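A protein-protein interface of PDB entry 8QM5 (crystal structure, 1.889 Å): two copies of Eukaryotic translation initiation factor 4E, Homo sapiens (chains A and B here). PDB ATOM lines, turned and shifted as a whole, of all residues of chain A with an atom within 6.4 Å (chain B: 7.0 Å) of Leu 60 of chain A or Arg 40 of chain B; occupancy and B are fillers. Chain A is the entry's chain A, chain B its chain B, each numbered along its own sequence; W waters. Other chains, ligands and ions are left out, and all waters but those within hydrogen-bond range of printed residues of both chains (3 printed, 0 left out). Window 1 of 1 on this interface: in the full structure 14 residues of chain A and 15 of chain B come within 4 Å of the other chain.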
ATOM      1  N   ALA A  42      -0.762   9.164 -10.509  1.00  0.00           N
ATOM      2  CA  ALA A  42      -1.643   9.892 -11.386  1.00  0.00           C
ATOM      3  C   ALA A  42      -2.943  10.104 -10.659  1.00  0.00           C
ATOM      4  O   ALA A  42      -3.544   9.144 -10.099  1.00  0.00           O
ATOM      5  CB  ALA A  42      -1.880   9.103 -12.689  1.00  0.00           C
ATOM      6  N   LEU A  43      -3.393  11.337 -10.659  1.00  0.00           N
ATOM      7  CA  LEU A  43      -4.706  11.709 -10.167  1.00  0.00           C
ATOM      8  C   LEU A  43      -5.710  11.729 -11.345  1.00  0.00           C
ATOM      9  O   LEU A  43      -5.487  12.402 -12.370  1.00  0.00           O
ATOM     10  CB  LEU A  43      -4.650  13.107  -9.506  1.00  0.00           C
ATOM     11  CG  LEU A  43      -5.996  13.553  -8.903  1.00  0.00           C
ATOM     12  CD1 LEU A  43      -6.388  12.719  -7.746  1.00  0.00           C
ATOM     13  CD2 LEU A  43      -5.954  14.993  -8.496  1.00  0.00           C
ATOM     14  N   TRP A  44      -6.781  11.005 -11.200  1.00  0.00           N
ATOM     15  CA  TRP A  44      -7.871  10.888 -12.120  1.00  0.00           C
ATOM     16  C   TRP A  44      -9.154  11.476 -11.559  1.00  0.00           C
ATOM     17  O   TRP A  44      -9.376  11.530 -10.329  1.00  0.00           O
ATOM     18  CB  TRP A  44      -8.124   9.441 -12.493  1.00  0.00           C
ATOM     19  CG  TRP A  44      -6.948   8.660 -12.988  1.00  0.00           C
ATOM     20  CD1 TRP A  44      -5.879   8.191 -12.278  1.00  0.00           C
ATOM     21  CD2 TRP A  44      -6.775   8.208 -14.321  1.00  0.00           C
ATOM     22  NE1 TRP A  44      -5.065   7.448 -13.093  1.00  0.00           N
ATOM     23  CE2 TRP A  44      -5.549   7.496 -14.367  1.00  0.00           C
ATOM     24  CE3 TRP A  44      -7.499   8.406 -15.499  1.00  0.00           C
ATOM     25  CZ2 TRP A  44      -5.070   6.903 -15.533  1.00  0.00           C
ATOM     26  CZ3 TRP A  44      -7.006   7.842 -16.673  1.00  0.00           C
ATOM     27  CH2 TRP A  44      -5.796   7.111 -16.681  1.00  0.00           C
ATOM     28  N   PHE A  45     -10.018  11.911 -12.448  1.00  0.00           N
ATOM     29  CA  PHE A  45     -11.325  12.426 -12.132  1.00  0.00           C
ATOM     30  C   PHE A  45     -12.360  11.852 -13.083  1.00  0.00           C
ATOM     31  O   PHE A  45     -12.070  11.699 -14.273  1.00  0.00           O
ATOM     32  CB  PHE A  45     -11.263  13.961 -12.280  1.00  0.00           C
ATOM     33  CG  PHE A  45     -12.541  14.724 -12.111  1.00  0.00           C
ATOM     34  CD1 PHE A  45     -13.179  14.769 -10.885  1.00  0.00           C
ATOM     35  CD2 PHE A  45     -13.093  15.418 -13.164  1.00  0.00           C
ATOM     36  CE1 PHE A  45     -14.355  15.483 -10.722  1.00  0.00           C
ATOM     37  CE2 PHE A  45     -14.259  16.136 -13.005  1.00  0.00           C
ATOM     38  CZ  PHE A  45     -14.897  16.162 -11.785  1.00  0.00           C
ATOM     39  N   GLN A  55     -16.356   6.953 -21.017  1.00  0.00           N
ATOM     40  CA  GLN A  55     -14.973   6.979 -21.477  1.00  0.00           C
ATOM     41  C   GLN A  55     -14.532   8.456 -21.677  1.00  0.00           C
ATOM     42  O   GLN A  55     -13.427   8.784 -21.282  1.00  0.00           O
ATOM     43  CB  GLN A  55     -14.706   6.104 -22.724  1.00  0.00           C
ATOM     44  CG  GLN A  55     -13.168   5.890 -22.962  1.00  0.00           C
ATOM     45  CD  GLN A  55     -12.713   4.982 -24.103  1.00  0.00           C
ATOM     46  OE1 GLN A  55     -13.392   4.810 -25.134  1.00  0.00           O
ATOM     47  NE2 GLN A  55     -11.517   4.383 -23.924  1.00  0.00           N
ATOM     48  N   LEU A  58     -14.044  10.102 -17.984  1.00  0.00           N
ATOM     49  CA  LEU A  58     -12.894   9.723 -17.167  1.00  0.00           C
ATOM     50  C   LEU A  58     -11.657  10.445 -17.723  1.00  0.00           C
ATOM     51  O   LEU A  58     -11.289  10.277 -18.894  1.00  0.00           O
ATOM     52  CB  LEU A  58     -12.667   8.212 -17.171  1.00  0.00           C
ATOM     53  CG  LEU A  58     -11.419   7.724 -16.387  1.00  0.00           C
ATOM     54  CD1 LEU A  58     -11.487   8.105 -14.913  1.00  0.00           C
ATOM     55  CD2 LEU A  58     -11.258   6.262 -16.549  1.00  0.00           C
ATOM     56  N   ARG A  59     -11.056  11.247 -16.894  1.00  0.00           N
ATOM     57  CA  ARG A  59      -9.954  12.143 -17.214  1.00  0.00           C
ATOM     58  C   ARG A  59      -8.760  11.979 -16.267  1.00  0.00           C
ATOM     59  O   ARG A  59      -8.954  11.846 -15.037  1.00  0.00           O
ATOM     60  CB  ARG A  59     -10.435  13.582 -17.137  1.00  0.00           C
ATOM     61  CG  ARG A  59     -10.734  14.212 -18.493  1.00  0.00           C
ATOM     62  CD  ARG A  59     -10.618  15.730 -18.453  1.00  0.00           C
ATOM     63  NE  ARG A  59      -9.241  16.149 -18.149  1.00  0.00           N
ATOM     64  CZ  ARG A  59      -8.873  17.404 -17.898  1.00  0.00           C
ATOM     65  NH1 ARG A  59      -9.770  18.387 -17.926  1.00  0.00           N
ATOM     66  NH2 ARG A  59      -7.605  17.686 -17.620  1.00  0.00           N
ATOM     67  N   LEU A  60      -7.543  11.976 -16.828  1.00  0.00           N
ATOM     68  CA  LEU A  60      -6.300  12.064 -16.070  1.00  0.00           C
ATOM     69  C   LEU A  60      -5.899  13.529 -15.862  1.00  0.00           C
ATOM     70  O   LEU A  60      -5.593  14.222 -16.834  1.00  0.00           O
ATOM     71  CB  LEU A  60      -5.187  11.239 -16.730  1.00  0.00           C
ATOM     72  CG  LEU A  60      -3.940  10.935 -15.860  1.00  0.00           C
ATOM     73  CD1 LEU A  60      -3.289   9.625 -16.308  1.00  0.00           C
ATOM     74  CD2 LEU A  60      -2.962  12.054 -15.972  1.00  0.00           C
ATOM     75  N   ILE A  61      -5.919  14.005 -14.606  1.00  0.00           N
ATOM     76  CA  ILE A  61      -5.730  15.411 -14.190  1.00  0.00           C
ATOM     77  C   ILE A  61      -4.245  15.741 -14.233  1.00  0.00           C
ATOM     78  O   ILE A  61      -3.838  16.679 -14.923  1.00  0.00           O
ATOM     79  CB  ILE A  61      -6.340  15.682 -12.783  1.00  0.00           C
ATOM     80  CG1 ILE A  61      -7.867  15.443 -12.755  1.00  0.00           C
ATOM     81  CG2 ILE A  61      -5.977  17.062 -12.277  1.00  0.00           C
ATOM     82  CD1 ILE A  61      -8.687  16.130 -13.909  1.00  0.00           C
ATOM     83  N   SER A  62      -3.413  14.975 -13.506  1.00  0.00           N
ATOM     84  CA  SER A  62      -1.999  15.276 -13.417  1.00  0.00           C
ATOM     85  C   SER A  62      -1.217  14.065 -12.839  1.00  0.00           C
ATOM     86  O   SER A  62      -1.779  13.162 -12.196  1.00  0.00           O
ATOM     87  CB  SER A  62      -1.778  16.517 -12.539  1.00  0.00           C
ATOM     88  OG  SER A  62      -0.472  17.046 -12.700  1.00  0.00           O
ATOM     89  N   LYS A  63       0.071  14.051 -13.114  1.00  0.00           N
ATOM     90  CA  LYS A  63       0.982  13.043 -12.552  1.00  0.00           C
ATOM     91  C   LYS A  63       2.066  13.743 -11.750  1.00  0.00           C
ATOM     92  O   LYS A  63       2.451  14.854 -12.091  1.00  0.00           O
ATOM     93  CB  LYS A  63       1.591  12.181 -13.647  1.00  0.00           C
ATOM     94  CG  LYS A  63       0.536  11.538 -14.566  1.00  0.00           C
ATOM     95  CD  LYS A  63       1.160  10.480 -15.426  1.00  0.00           C
ATOM     96  CE  LYS A  63       0.233   9.654 -16.283  1.00  0.00           C
ATOM     97  NZ  LYS A  63       0.976   8.658 -17.128  1.00  0.00           N
ATOM     98  N   ASP A  94       1.370   5.151 -11.551  1.00  0.00           N
ATOM     99  CA  ASP A  94       1.552   5.465 -12.984  1.00  0.00           C
ATOM    100  C   ASP A  94       1.467   4.160 -13.798  1.00  0.00           C
ATOM    101  O   ASP A  94       2.113   3.175 -13.431  1.00  0.00           O
ATOM    102  CB  ASP A  94       2.891   6.213 -13.178  1.00  0.00           C
ATOM    103  CG  ASP A  94       3.049   6.930 -14.503  1.00  0.00           C
ATOM    104  OD1 ASP A  94       2.046   7.110 -15.187  1.00  0.00           O
ATOM    105  OD2 ASP A  94       4.191   7.316 -14.844  1.00  0.00           O
ATOM    106  N   GLU A  97      -4.807   2.061 -14.821  1.00  0.00           N
ATOM    107  CA  GLU A  97      -6.061   2.761 -14.961  1.00  0.00           C
ATOM    108  C   GLU A  97      -6.985   2.453 -13.764  1.00  0.00           C
ATOM    109  O   GLU A  97      -6.951   1.324 -13.261  1.00  0.00           O
ATOM    110  CB  GLU A  97      -6.746   2.400 -16.258  1.00  0.00           C
ATOM    111  CG  GLU A  97      -5.903   2.766 -17.460  1.00  0.00           C
ATOM    112  CD  GLU A  97      -6.686   2.683 -18.770  1.00  0.00           C
ATOM    113  OE1 GLU A  97      -7.687   1.935 -18.840  1.00  0.00           O
ATOM    114  OE2 GLU A  97      -6.288   3.380 -19.720  1.00  0.00           O
ATOM    115  N   LEU B  37       3.420   7.390 -20.442  1.00  0.00           N
ATOM    116  CA  LEU B  37       3.523   8.654 -21.125  1.00  0.00           C
ATOM    117  C   LEU B  37       3.354   9.823 -20.172  1.00  0.00           C
ATOM    118  O   LEU B  37       2.711   9.704 -19.111  1.00  0.00           O
ATOM    119  CB  LEU B  37       2.436   8.693 -22.209  1.00  0.00           C
ATOM    120  CG  LEU B  37       2.518   7.636 -23.319  1.00  0.00           C
ATOM    121  CD1 LEU B  37       1.358   7.736 -24.302  1.00  0.00           C
ATOM    122  CD2 LEU B  37       3.876   7.647 -24.022  1.00  0.00           C
ATOM    123  N   GLN B  38       3.902  10.988 -20.543  1.00  0.00           N
ATOM    124  CA  GLN B  38       3.691  12.239 -19.780  1.00  0.00           C
ATOM    125  C   GLN B  38       2.206  12.563 -19.685  1.00  0.00           C
ATOM    126  O   GLN B  38       1.722  12.976 -18.623  1.00  0.00           O
ATOM    127  CB  GLN B  38       4.469  13.365 -20.449  1.00  0.00           C
ATOM    128  CG  GLN B  38       4.381  14.727 -19.784  1.00  0.00           C
ATOM    129  CD  GLN B  38       5.043  14.787 -18.420  1.00  0.00           C
ATOM    130  OE1 GLN B  38       5.918  13.975 -18.067  1.00  0.00           O
ATOM    131  NE2 GLN B  38       4.648  15.774 -17.630  1.00  0.00           N
ATOM    132  N   ASN B  39       1.477  12.358 -20.801  1.00  0.00           N
ATOM    133  CA  ASN B  39       0.077  12.746 -20.912  1.00  0.00           C
ATOM    134  C   ASN B  39      -0.759  11.539 -21.256  1.00  0.00           C
ATOM    135  O   ASN B  39      -0.269  10.574 -21.878  1.00  0.00           O
ATOM    136  CB  ASN B  39      -0.101  13.813 -22.019  1.00  0.00           C
ATOM    137  CG  ASN B  39       0.383  15.176 -21.565  1.00  0.00           C
ATOM    138  OD1 ASN B  39      -0.261  15.842 -20.772  1.00  0.00           O
ATOM    139  ND2 ASN B  39       1.519  15.599 -22.020  1.00  0.00           N
ATOM    140  N   ARG B  40      -2.044  11.609 -20.865  1.00  0.00           N
ATOM    141  CA  ARG B  40      -3.030  10.739 -21.423  1.00  0.00           C
ATOM    142  C   ARG B  40      -3.516  11.381 -22.715  1.00  0.00           C
ATOM    143  O   ARG B  40      -3.658  12.585 -22.812  1.00  0.00           O
ATOM    144  CB  ARG B  40      -4.131  10.399 -20.427  1.00  0.00           C
ATOM    145  CG  ARG B  40      -5.149   9.399 -20.894  1.00  0.00           C
ATOM    146  CD  ARG B  40      -5.973   8.950 -19.707  1.00  0.00           C
ATOM    147  NE  ARG B  40      -6.859   7.785 -19.877  1.00  0.00           N
ATOM    148  CZ  ARG B  40      -8.201   7.790 -19.795  1.00  0.00           C
ATOM    149  NH1 ARG B  40      -8.864   8.924 -19.567  1.00  0.00           N
ATOM    150  NH2 ARG B  40      -8.883   6.662 -19.926  1.00  0.00           N
ATOM    151  N   TRP B  41      -3.721  10.551 -23.718  1.00  0.00           N
ATOM    152  CA  TRP B  41      -4.180  10.959 -25.068  1.00  0.00           C
ATOM    153  C   TRP B  41      -5.475  10.200 -25.435  1.00  0.00           C
ATOM    154  O   TRP B  41      -5.740   9.106 -24.973  1.00  0.00           O
ATOM    155  CB  TRP B  41      -3.118  10.621 -26.162  1.00  0.00           C
ATOM    156  CG  TRP B  41      -1.809  11.269 -25.931  1.00  0.00           C
ATOM    157  CD1 TRP B  41      -0.834  10.855 -25.080  1.00  0.00           C
ATOM    158  CD2 TRP B  41      -1.402  12.553 -26.411  1.00  0.00           C
ATOM    159  NE1 TRP B  41       0.187  11.757 -25.073  1.00  0.00           N
ATOM    160  CE2 TRP B  41      -0.143  12.824 -25.845  1.00  0.00           C
ATOM    161  CE3 TRP B  41      -1.994  13.512 -27.217  1.00  0.00           C
ATOM    162  CZ2 TRP B  41       0.546  14.009 -26.084  1.00  0.00           C
ATOM    163  CZ3 TRP B  41      -1.282  14.650 -27.526  1.00  0.00           C
ATOM    164  CH2 TRP B  41      -0.020  14.895 -26.951  1.00  0.00           C
ATOM    165  N   ALA B  42      -6.277  10.820 -26.292  1.00  0.00           N
ATOM    166  CA  ALA B  42      -7.519  10.292 -26.778  1.00  0.00           C
ATOM    167  C   ALA B  42      -7.480  10.328 -28.295  1.00  0.00           C
ATOM    168  O   ALA B  42      -7.159  11.365 -28.905  1.00  0.00           O
ATOM    169  CB  ALA B  42      -8.673  11.120 -26.245  1.00  0.00           C
ATOM    170  N   SER B  62     -10.720   5.675 -28.324  1.00  0.00           N
ATOM    171  CA  SER B  62     -10.039   5.113 -27.143  1.00  0.00           C
ATOM    172  C   SER B  62      -9.086   6.142 -26.507  1.00  0.00           C
ATOM    173  O   SER B  62      -8.692   7.135 -27.126  1.00  0.00           O
ATOM    174  CB  SER B  62      -9.297   3.839 -27.539  1.00  0.00           C
ATOM    175  OG  SER B  62      -8.918   3.068 -26.411  1.00  0.00           O
ATOM    176  N   LYS B  63      -8.738   5.910 -25.265  1.00  0.00           N
ATOM    177  CA  LYS B  63      -7.735   6.692 -24.555  1.00  0.00           C
ATOM    178  C   LYS B  63      -6.603   5.791 -24.075  1.00  0.00           C
ATOM    179  O   LYS B  63      -6.841   4.624 -23.755  1.00  0.00           O
ATOM    180  CB  LYS B  63      -8.361   7.430 -23.354  1.00  0.00           C
ATOM    181  CG  LYS B  63      -9.554   8.288 -23.751  1.00  0.00           C
ATOM    182  CD  LYS B  63      -9.914   9.231 -22.608  1.00  0.00           C
ATOM    183  CE  LYS B  63     -11.005  10.241 -22.880  1.00  0.00           C
ATOM    184  NZ  LYS B  63     -11.316  11.077 -21.650  1.00  0.00           N
ATOM    185  N   PHE B  64      -5.370   6.329 -24.018  1.00  0.00           N
ATOM    186  CA  PHE B  64      -4.207   5.601 -23.524  1.00  0.00           C
ATOM    187  C   PHE B  64      -3.196   6.555 -22.860  1.00  0.00           C
ATOM    188  O   PHE B  64      -3.180   7.749 -23.151  1.00  0.00           O
ATOM    189  CB  PHE B  64      -3.530   4.827 -24.667  1.00  0.00           C
ATOM    190  CG  PHE B  64      -3.049   5.745 -25.770  1.00  0.00           C
ATOM    191  CD1 PHE B  64      -3.894   6.111 -26.808  1.00  0.00           C
ATOM    192  CD2 PHE B  64      -1.761   6.265 -25.756  1.00  0.00           C
ATOM    193  CE1 PHE B  64      -3.446   6.936 -27.820  1.00  0.00           C
ATOM    194  CE2 PHE B  64      -1.354   7.170 -26.724  1.00  0.00           C
ATOM    195  CZ  PHE B  64      -2.177   7.456 -27.784  1.00  0.00           C
ATOM    196  N   ASP B  65      -2.352   6.019 -21.974  1.00  0.00           N
ATOM    197  CA  ASP B  65      -1.258   6.787 -21.385  1.00  0.00           C
ATOM    198  C   ASP B  65      -0.007   5.967 -21.177  1.00  0.00           C
ATOM    199  O   ASP B  65       0.805   6.282 -20.290  1.00  0.00           O
ATOM    200  CB  ASP B  65      -1.644   7.570 -20.129  1.00  0.00           C
ATOM    201  CG  ASP B  65      -1.808   6.734 -18.923  1.00  0.00           C
ATOM    202  OD1 ASP B  65      -2.437   5.681 -19.035  1.00  0.00           O
ATOM    203  OD2 ASP B  65      -1.299   7.143 -17.847  1.00  0.00           O
ATOM    204  N   THR B  66       0.157   4.900 -22.017  1.00  0.00           N
ATOM    205  CA  THR B  66       1.378   4.116 -22.103  1.00  0.00           C
ATOM    206  C   THR B  66       1.760   3.917 -23.553  1.00  0.00           C
ATOM    207  O   THR B  66       0.912   3.944 -24.460  1.00  0.00           O
ATOM    208  CB  THR B  66       1.320   2.753 -21.333  1.00  0.00           C
ATOM    209  OG1 THR B  66       0.745   1.789 -22.164  1.00  0.00           O
ATOM    210  CG2 THR B  66       0.637   2.862 -19.972  1.00  0.00           C
ATOM    211  N   PHE B  92      -5.691  13.827 -29.383  1.00  0.00           N
ATOM    212  CA  PHE B  92      -5.607  14.998 -28.503  1.00  0.00           C
ATOM    213  C   PHE B  92      -5.339  14.674 -27.079  1.00  0.00           C
ATOM    214  O   PHE B  92      -5.681  13.579 -26.575  1.00  0.00           O
ATOM    215  CB  PHE B  92      -6.889  15.876 -28.611  1.00  0.00           C
ATOM    216  CG  PHE B  92      -6.852  16.841 -29.754  1.00  0.00           C
ATOM    217  CD1 PHE B  92      -6.902  16.387 -31.079  1.00  0.00           C
ATOM    218  CD2 PHE B  92      -6.739  18.197 -29.527  1.00  0.00           C
ATOM    219  CE1 PHE B  92      -6.795  17.276 -32.138  1.00  0.00           C
ATOM    220  CE2 PHE B  92      -6.633  19.071 -30.592  1.00  0.00           C
ATOM    221  CZ  PHE B  92      -6.685  18.609 -31.881  1.00  0.00           C
ATOM    222  N   LYS B  93      -4.697  15.606 -26.375  1.00  0.00           N
ATOM    223  CA  LYS B  93      -4.478  15.416 -24.934  1.00  0.00           C
ATOM    224  C   LYS B  93      -5.848  15.214 -24.231  1.00  0.00           C
ATOM    225  O   LYS B  93      -6.881  15.800 -24.618  1.00  0.00           O
ATOM    226  CB  LYS B  93      -3.701  16.563 -24.306  1.00  0.00           C
ATOM    227  CG  LYS B  93      -2.280  16.630 -24.734  1.00  0.00           C
ATOM    228  CD  LYS B  93      -1.619  17.775 -24.175  1.00  0.00           C
ATOM    229  CE  LYS B  93      -0.160  17.726 -24.469  1.00  0.00           C
ATOM    230  NZ  LYS B  93       0.478  18.961 -24.082  1.00  0.00           N
ATOM    231  N   ASP B  94      -5.861  14.380 -23.232  1.00  0.00           N
ATOM    232  CA  ASP B  94      -7.074  14.031 -22.473  1.00  0.00           C
ATOM    233  C   ASP B  94      -7.731  15.355 -21.938  1.00  0.00           C
ATOM    234  O   ASP B  94      -7.043  16.189 -21.373  1.00  0.00           O
ATOM    235  CB  ASP B  94      -6.717  13.052 -21.347  1.00  0.00           C
ATOM    236  CG  ASP B  94      -7.878  12.326 -20.713  1.00  0.00           C
ATOM    237  OD1 ASP B  94      -8.989  12.376 -21.277  1.00  0.00           O
ATOM    238  OD2 ASP B  94      -7.656  11.675 -19.669  1.00  0.00           O
ATOM    239  N   GLY B  95      -9.021  15.532 -22.196  1.00  0.00           N
ATOM    240  CA  GLY B  95      -9.705  16.763 -21.804  1.00  0.00           C
ATOM    241  C   GLY B  95      -9.758  17.842 -22.860  1.00  0.00           C
ATOM    242  O   GLY B  95     -10.344  18.898 -22.605  1.00  0.00           O
HETATM  243  O   HOH W   1      -5.211   5.521 -20.094  1.00  0.00           O
HETATM  244  O   HOH W   2     -11.633   6.850 -20.571  1.00  0.00           O
HETATM  245  O   HOH W   3      -5.689   1.982 -22.635  1.00  0.00           O
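Leu 60 of chain A touches just these residues of chain B: Arg 40, Asp 65 and Asp 94. Arg 40 of chain B touches just these residues of chain A: Trp 44 (3.2 Å), Leu 58 (2.9 Å) and Leu 60 (3.8 Å). Of the printed residues of chain B, Leu 58 of chain A touches Arg 40, Lys 63 and Asp 94. Printed residues of chain A within 4 Å of Asp 65 of chain B: Leu 60 (3.5 Å) and Lys 63 (2.8 Å). Printed residues of chain B within 4 Å of Lys 63 of chain A: Leu 37 (2.8 Å) and Asp 65 (2.8 Å). Of the printed residues of chain A, Asp 94 of chain B touches Leu 58, Arg 59 and Leu 60. The nearest residue of chain A that does not touch Arg 40 of chain B is Arg 59 of chain A (4.1 Å).
Trp 44 of chain A touches Arg 40 of chain B (CZ3 to NE, 3.2 Å). CA of Ser 62 of chain B touches NE2 of Gln 55 of chain A, 3.6 Å away. Asp 94 of chain B touches Leu 58 of chain A (OD1 to O, 3.9 Å). Arg 59 of chain A touches Asp 94 of chain B (CA to OD2, 3.4 Å). Arg 59 of chain A touches Gly 95 of chain B (CD to CA, 3.6 Å). Leu 60 of chain A touches Arg 40 of chain B (CB to CD, 3.8 Å). Leu 60 of chain A touches Asp 65 of chain B.
The side-chain amino group (NZ) of Lys 63 of chain B lies within hydrogen-bond range of the backbone carbonyl oxygen (O) of Gln 55 of chain A, at 3.1 Å. NH1 of Arg 40 of chain B is in hydrogen-bond range of O of Leu 58 of chain A (2.9 Å). O of Leu 58 of chain A is in hydrogen-bond range of NZ of Lys 63 of chain B, at 2.9 Å. The backbone NH (N) of Leu 60 of chain A lies within hydrogen-bond range of the side-chain carboxylate (OD2) of Asp 94 of chain B, 2.9 Å away. The side-chain amino group of Lys 63 of chain A is in hydrogen-bond range of the backbone carbonyl oxygen of Leu 37 of chain B (2.8 Å). The side-chain amino group (NZ) of Lys 63 of chain A lies within salt-bridge range of the side-chain carboxylate (OD2) of Asp 65 of chain B, 2.8 Å away.
Printed residues of chain A that touch a printed residue of chain B: Trp 44, Gln 55, Leu 58, Arg 59, Leu 60 and Lys 63. Hydrophobic or aromatic side chains of chain A that line the printed part of chain B: Trp 44 and Leu 60. Of the 15 printed residues of chain B, 7 touch a printed residue of chain A. Among the printed residues, 13 pairs touch across the chains.
O of Arg 59 of chain A is in hydrogen-bond range of N of Phe 45 of chain A (2.8 Å). NZ of Lys 63 of chain A lies within salt-bridge range of OD1 of Asp 94 of chain A, 2.7 Å away. The backbone NH (N) of Leu 37 of chain B sits at hydrogen-bond distance from the backbone carbonyl oxygen (O) of Asp 65 of chain B, at 2.8 Å. The side-chain carboxylate (OD2) of Asp 94 of chain B is in salt-bridge range of the guanidinium group (NH1) of Arg 40 of chain B (3.0 Å). The side-chain amino group (NZ) of Lys 63 of chain B is in salt-bridge range of the side-chain carboxylate (OD1) of Asp 94 of chain B, 2.7 Å away.
4 positions are printed for both chains.
Water W1 lies within hydrogen-bond range of the side-chain carboxylate (OE2) of Glu 97 of chain A, the guanidinium group (NE) of Arg 40 of chain B and the side-chain carboxylate (OD1) of Asp 65 of chain B. Water W2 lies within hydrogen-bond range of the backbone carbonyl oxygen (O) of Gln 55 of chain A and the guanidinium group (NH2) of Arg 40 of chain B. Water W3 bridges the backbone carbonyl oxygen (O) of Lys 63 of chain B and the side-chain carboxylate (OE2) of Glu 97 of chain A.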
